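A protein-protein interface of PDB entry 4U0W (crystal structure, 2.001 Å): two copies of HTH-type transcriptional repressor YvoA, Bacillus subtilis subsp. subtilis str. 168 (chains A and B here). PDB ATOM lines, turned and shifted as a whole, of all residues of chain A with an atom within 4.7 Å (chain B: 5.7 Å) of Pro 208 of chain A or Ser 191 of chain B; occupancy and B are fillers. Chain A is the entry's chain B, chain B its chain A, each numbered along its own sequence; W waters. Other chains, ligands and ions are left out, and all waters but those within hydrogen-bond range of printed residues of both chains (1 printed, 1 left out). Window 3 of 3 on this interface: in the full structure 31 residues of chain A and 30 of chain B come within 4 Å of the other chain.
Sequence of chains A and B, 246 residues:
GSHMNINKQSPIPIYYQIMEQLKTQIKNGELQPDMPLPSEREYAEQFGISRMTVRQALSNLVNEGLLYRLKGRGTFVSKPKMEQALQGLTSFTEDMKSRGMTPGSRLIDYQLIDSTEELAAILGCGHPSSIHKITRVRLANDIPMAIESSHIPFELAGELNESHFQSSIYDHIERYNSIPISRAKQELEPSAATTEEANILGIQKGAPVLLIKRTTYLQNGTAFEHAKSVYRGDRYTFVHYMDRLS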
ATOM      1  N   SER A 191     -25.060  -8.409  29.563  1.00  0.00           N
ATOM      2  CA  SER A 191     -25.979  -7.315  29.781  1.00  0.00           C
ATOM      3  C   SER A 191     -27.310  -7.568  29.113  1.00  0.00           C
ATOM      4  O   SER A 191     -27.487  -8.553  28.410  1.00  0.00           O
ATOM      5  CB  SER A 191     -25.377  -5.997  29.253  1.00  0.00           C
ATOM      6  OG  SER A 191     -26.003  -4.891  29.901  1.00  0.00           O
ATOM      7  N   GLY A 206     -34.126  -5.620  26.025  1.00  0.00           N
ATOM      8  CA  GLY A 206     -33.731  -6.432  27.161  1.00  0.00           C
ATOM      9  C   GLY A 206     -33.116  -7.776  26.794  1.00  0.00           C
ATOM     10  O   GLY A 206     -32.716  -8.533  27.680  1.00  0.00           O
ATOM     11  N   ALA A 207     -33.034  -8.075  25.500  1.00  0.00           N
ATOM     12  CA  ALA A 207     -32.385  -9.307  25.036  1.00  0.00           C
ATOM     13  C   ALA A 207     -30.925  -9.341  25.476  1.00  0.00           C
ATOM     14  O   ALA A 207     -30.279  -8.286  25.621  1.00  0.00           O
ATOM     15  CB  ALA A 207     -32.489  -9.442  23.501  1.00  0.00           C
ATOM     16  N   PRO A 208     -30.408 -10.550  25.728  1.00  0.00           N
ATOM     17  CA  PRO A 208     -29.030 -10.756  26.176  1.00  0.00           C
ATOM     18  C   PRO A 208     -27.983 -10.271  25.177  1.00  0.00           C
ATOM     19  O   PRO A 208     -28.064 -10.587  23.989  1.00  0.00           O
ATOM     20  CB  PRO A 208     -28.942 -12.279  26.354  1.00  0.00           C
ATOM     21  CG  PRO A 208     -30.367 -12.696  26.642  1.00  0.00           C
ATOM     22  CD  PRO A 208     -31.204 -11.798  25.795  1.00  0.00           C
ATOM     23  N   VAL A 209     -27.018  -9.494  25.674  1.00  0.00           N
ATOM     24  CA  VAL A 209     -25.882  -9.064  24.876  1.00  0.00           C
ATOM     25  C   VAL A 209     -24.619  -9.161  25.707  1.00  0.00           C
ATOM     26  O   VAL A 209     -24.677  -9.160  26.933  1.00  0.00           O
ATOM     27  CB  VAL A 209     -26.057  -7.607  24.369  1.00  0.00           C
ATOM     28  CG1 VAL A 209     -27.234  -7.527  23.396  1.00  0.00           C
ATOM     29  CG2 VAL A 209     -26.242  -6.643  25.548  1.00  0.00           C
ATOM     30  N   LEU A 210     -23.481  -9.277  25.037  1.00  0.00           N
ATOM     31  CA  LEU A 210     -22.206  -9.183  25.713  1.00  0.00           C
ATOM     32  C   LEU A 210     -21.666  -7.754  25.586  1.00  0.00           C
ATOM     33  O   LEU A 210     -21.430  -7.253  24.484  1.00  0.00           O
ATOM     34  CB  LEU A 210     -21.192 -10.174  25.149  1.00  0.00           C
ATOM     35  CG  LEU A 210     -19.973 -10.432  26.048  1.00  0.00           C
ATOM     36  CD1 LEU A 210     -20.422 -11.036  27.371  1.00  0.00           C
ATOM     37  CD2 LEU A 210     -18.999 -11.363  25.365  1.00  0.00           C
ATOM     38  N   TYR A 231     -22.476  -6.814  21.740  1.00  0.00           N
ATOM     39  CA  TYR A 231     -22.598  -7.911  20.768  1.00  0.00           C
ATOM     40  C   TYR A 231     -23.843  -8.743  21.027  1.00  0.00           C
ATOM     41  O   TYR A 231     -24.139  -9.089  22.172  1.00  0.00           O
ATOM     42  CB  TYR A 231     -21.358  -8.806  20.801  1.00  0.00           C
ATOM     43  CG  TYR A 231     -20.255  -8.313  19.912  1.00  0.00           C
ATOM     44  CD1 TYR A 231     -19.591  -7.109  20.186  1.00  0.00           C
ATOM     45  CD2 TYR A 231     -19.881  -9.031  18.788  1.00  0.00           C
ATOM     46  CE1 TYR A 231     -18.595  -6.653  19.355  1.00  0.00           C
ATOM     47  CE2 TYR A 231     -18.882  -8.589  17.954  1.00  0.00           C
ATOM     48  CZ  TYR A 231     -18.240  -7.393  18.244  1.00  0.00           C
ATOM     49  OH  TYR A 231     -17.243  -6.952  17.412  1.00  0.00           O
ATOM     50  N   ARG A 232     -24.561  -9.064  19.954  1.00  0.00           N
ATOM     51  CA  ARG A 232     -25.799  -9.841  20.036  1.00  0.00           C
ATOM     52  C   ARG A 232     -25.584 -11.213  20.653  1.00  0.00           C
ATOM     53  O   ARG A 232     -24.838 -12.016  20.099  1.00  0.00           O
ATOM     54  CB  ARG A 232     -26.391 -10.043  18.651  1.00  0.00           C
ATOM     55  CG  ARG A 232     -27.136  -8.886  18.083  1.00  0.00           C
ATOM     56  CD  ARG A 232     -27.582  -9.260  16.686  1.00  0.00           C
ATOM     57  NE  ARG A 232     -28.757 -10.120  16.694  1.00  0.00           N
ATOM     58  CZ  ARG A 232     -29.501 -10.346  15.620  1.00  0.00           C
ATOM     59  NH1 ARG A 232     -29.170  -9.783  14.464  1.00  0.00           N
ATOM     60  NH2 ARG A 232     -30.570 -11.127  15.704  1.00  0.00           N
ATOM     61  N   GLY A 233     -26.255 -11.493  21.765  1.00  0.00           N
ATOM     62  CA  GLY A 233     -26.166 -12.811  22.369  1.00  0.00           C
ATOM     63  C   GLY A 233     -26.678 -13.912  21.443  1.00  0.00           C
ATOM     64  O   GLY A 233     -26.131 -15.015  21.417  1.00  0.00           O
ATOM     65  N   ASP A 234     -27.712 -13.613  20.664  1.00  0.00           N
ATOM     66  CA  ASP A 234     -28.388 -14.654  19.896  1.00  0.00           C
ATOM     67  C   ASP A 234     -27.627 -15.090  18.642  1.00  0.00           C
ATOM     68  O   ASP A 234     -28.024 -16.042  17.979  1.00  0.00           O
ATOM     69  CB  ASP A 234     -29.800 -14.205  19.509  1.00  0.00           C
ATOM     70  CG  ASP A 234     -29.810 -12.954  18.636  1.00  0.00           C
ATOM     71  OD1 ASP A 234     -28.831 -12.176  18.664  1.00  0.00           O
ATOM     72  OD2 ASP A 234     -30.808 -12.755  17.914  1.00  0.00           O
ATOM     73  N   GLU B 189     -21.566 -17.318  26.772  1.00  0.00           N
ATOM     74  CA  GLU B 189     -22.792 -16.755  26.226  1.00  0.00           C
ATOM     75  C   GLU B 189     -23.459 -15.909  27.302  1.00  0.00           C
ATOM     76  O   GLU B 189     -23.598 -16.353  28.442  1.00  0.00           O
ATOM     77  CB  GLU B 189     -23.739 -17.876  25.734  1.00  0.00           C
ATOM     78  CG  GLU B 189     -25.125 -17.403  25.329  1.00  0.00           C
ATOM     79  CD  GLU B 189     -26.030 -18.529  24.838  1.00  0.00           C
ATOM     80  OE1 GLU B 189     -27.261 -18.309  24.749  1.00  0.00           O
ATOM     81  OE2 GLU B 189     -25.517 -19.626  24.525  1.00  0.00           O
ATOM     82  N   PRO B 190     -23.872 -14.679  26.955  1.00  0.00           N
ATOM     83  CA  PRO B 190     -24.627 -13.871  27.915  1.00  0.00           C
ATOM     84  C   PRO B 190     -26.057 -14.362  27.963  1.00  0.00           C
ATOM     85  O   PRO B 190     -26.580 -14.805  26.939  1.00  0.00           O
ATOM     86  CB  PRO B 190     -24.564 -12.465  27.316  1.00  0.00           C
ATOM     87  CG  PRO B 190     -24.573 -12.758  25.806  1.00  0.00           C
ATOM     88  CD  PRO B 190     -23.661 -13.964  25.680  1.00  0.00           C
ATOM     89  N   SER B 191     -26.700 -14.279  29.110  1.00  0.00           N
ATOM     90  CA  SER B 191     -28.045 -14.789  29.176  1.00  0.00           C
ATOM     91  C   SER B 191     -28.799 -14.041  30.236  1.00  0.00           C
ATOM     92  O   SER B 191     -28.250 -13.152  30.894  1.00  0.00           O
ATOM     93  CB  SER B 191     -28.034 -16.302  29.469  1.00  0.00           C
ATOM     94  OG  SER B 191     -29.355 -16.798  29.584  1.00  0.00           O
ATOM     95  N   ALA B 192     -30.072 -14.377  30.385  1.00  0.00           N
ATOM     96  CA  ALA B 192     -30.889 -13.828  31.452  1.00  0.00           C
ATOM     97  C   ALA B 192     -31.130 -14.900  32.502  1.00  0.00           C
ATOM     98  O   ALA B 192     -31.513 -16.024  32.146  1.00  0.00           O
ATOM     99  CB  ALA B 192     -32.219 -13.306  30.896  1.00  0.00           C
ATOM    100  N   ALA B 193     -30.916 -14.571  33.782  1.00  0.00           N
ATOM    101  CA  ALA B 193     -31.140 -15.542  34.864  1.00  0.00           C
ATOM    102  C   ALA B 193     -32.577 -16.090  34.893  1.00  0.00           C
ATOM    103  O   ALA B 193     -33.543 -15.331  34.961  1.00  0.00           O
ATOM    104  CB  ALA B 193     -30.802 -14.917  36.218  1.00  0.00           C
ATOM    105  N   GLY B 206     -34.335 -12.735  35.404  1.00  0.00           N
ATOM    106  CA  GLY B 206     -33.946 -12.077  34.175  1.00  0.00           C
ATOM    107  C   GLY B 206     -32.657 -11.276  34.245  1.00  0.00           C
ATOM    108  O   GLY B 206     -32.193 -10.803  33.210  1.00  0.00           O
ATOM    109  N   ALA B 207     -32.064 -11.139  35.435  1.00  0.00           N
ATOM    110  CA  ALA B 207     -30.811 -10.394  35.564  1.00  0.00           C
ATOM    111  C   ALA B 207     -29.726 -11.007  34.680  1.00  0.00           C
ATOM    112  O   ALA B 207     -29.771 -12.202  34.373  1.00  0.00           O
ATOM    113  CB  ALA B 207     -30.358 -10.342  37.037  1.00  0.00           C
ATOM    114  N   PRO B 208     -28.763 -10.185  34.229  1.00  0.00           N
ATOM    115  CA  PRO B 208     -27.697 -10.641  33.331  1.00  0.00           C
ATOM    116  C   PRO B 208     -26.768 -11.682  33.959  1.00  0.00           C
ATOM    117  O   PRO B 208     -26.301 -11.465  35.073  1.00  0.00           O
ATOM    118  CB  PRO B 208     -26.921  -9.345  33.028  1.00  0.00           C
ATOM    119  CG  PRO B 208     -27.926  -8.258  33.215  1.00  0.00           C
ATOM    120  CD  PRO B 208     -28.765  -8.711  34.368  1.00  0.00           C
ATOM    121  N   VAL B 209     -26.516 -12.798  33.264  1.00  0.00           N
ATOM    122  CA  VAL B 209     -25.533 -13.778  33.726  1.00  0.00           C
ATOM    123  C   VAL B 209     -24.654 -14.261  32.591  1.00  0.00           C
ATOM    124  O   VAL B 209     -25.029 -14.191  31.420  1.00  0.00           O
ATOM    125  CB  VAL B 209     -26.215 -14.996  34.402  1.00  0.00           C
ATOM    126  CG1 VAL B 209     -27.008 -14.558  35.647  1.00  0.00           C
ATOM    127  CG2 VAL B 209     -27.124 -15.717  33.419  1.00  0.00           C
ATOM    128  N   LEU B 210     -23.468 -14.750  32.917  1.00  0.00           N
ATOM    129  CA  LEU B 210     -22.652 -15.350  31.891  1.00  0.00           C
ATOM    130  C   LEU B 210     -22.821 -16.881  31.925  1.00  0.00           C
ATOM    131  O   LEU B 210     -22.539 -17.522  32.937  1.00  0.00           O
ATOM    132  CB  LEU B 210     -21.191 -14.986  32.056  1.00  0.00           C
ATOM    133  CG  LEU B 210     -20.422 -15.244  30.763  1.00  0.00           C
ATOM    134  CD1 LEU B 210     -21.016 -14.354  29.650  1.00  0.00           C
ATOM    135  CD2 LEU B 210     -18.940 -14.976  30.974  1.00  0.00           C
ATOM    136  N   LEU B 211     -23.303 -17.429  30.817  1.00  0.00           N
ATOM    137  CA  LEU B 211     -23.399 -18.883  30.604  1.00  0.00           C
ATOM    138  C   LEU B 211     -22.077 -19.417  30.148  1.00  0.00           C
ATOM    139  O   LEU B 211     -21.575 -19.002  29.108  1.00  0.00           O
ATOM    140  CB  LEU B 211     -24.455 -19.205  29.544  1.00  0.00           C
ATOM    141  CG  LEU B 211     -25.656 -19.961  30.054  1.00  0.00           C
ATOM    142  CD1 LEU B 211     -26.366 -19.025  30.990  1.00  0.00           C
ATOM    143  CD2 LEU B 211     -26.535 -20.414  28.881  1.00  0.00           C
HETATM  144  O   HOH W   1     -33.529  -9.719  30.651  1.00  0.00           O
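Water W1 bridges O of Gly 206 of chain B (3.1 Å) and O of Gly 206 of chain A (3.3 Å).
Of the 11 printed residues of chain B, 3 touch a printed residue of chain A. Hydrophobic or aromatic side chains of chain B within 4 Å of the printed part of chain A: Pro 190 and Pro 208. Hydrophobic or aromatic side chains of chain A within 4 Å of the printed part of chain B: Pro 208.
Ser 191 of chain A touches Pro 208 of chain B, and with the chains exchanged Pro 208 of chain A touches Ser 191 of chain B. 6 positions are printed for both chains.
Printed residues of chain B within 4 Å of Ser 191 of chain A: Pro 208. Printed residues of chain B within 4 Å of Val 209 of chain A: Pro 190 (3.3 Å). Printed residues of chain B within 4 Å of Leu 210 of chain A: Pro 190 (3.7 Å). Of chain A, only Pro 208 comes within 4 Å of Ser 191 of chain B. Ala 193 of chain B touches none of the printed residues of chain A. Gly 206 of chain B touches none of the printed residues of chain A. The nearest printed residue of chain A that does not touch Ser 191 of chain B is Ser 191 of chain A (5.3 Å).
Among the printed residues, pairs that only touch across the chains: Ser 191 of chain A with Pro 208 of chain B, Pro 208 of chain A with Pro 190 of chain B, Pro 208 of chain A with Ser 191 of chain B, Val 209 of chain A with Pro 190 of chain B, Leu 210 of chain A with Pro 190 of chain B and Gly 233 of chain A with Pro 190 of chain B.
The backbone NH (N) of Ser 191 of chain B sits at hydrogen-bond distance from the backbone carbonyl oxygen (O) of Val 209 of chain B, 2.9 Å away. The backbone NH (N) of Ser 191 of chain A is in hydrogen-bond range of the backbone carbonyl oxygen (O) of Val 209 of chain A (2.8 Å). O of Pro 208 of chain A is in hydrogen-bond range of N of Gly 233 of chain A (3.0 Å). The backbone NH of Leu 210 of chain A sits at hydrogen-bond distance from the backbone carbonyl oxygen of Tyr 231 of chain A (2.9 Å).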
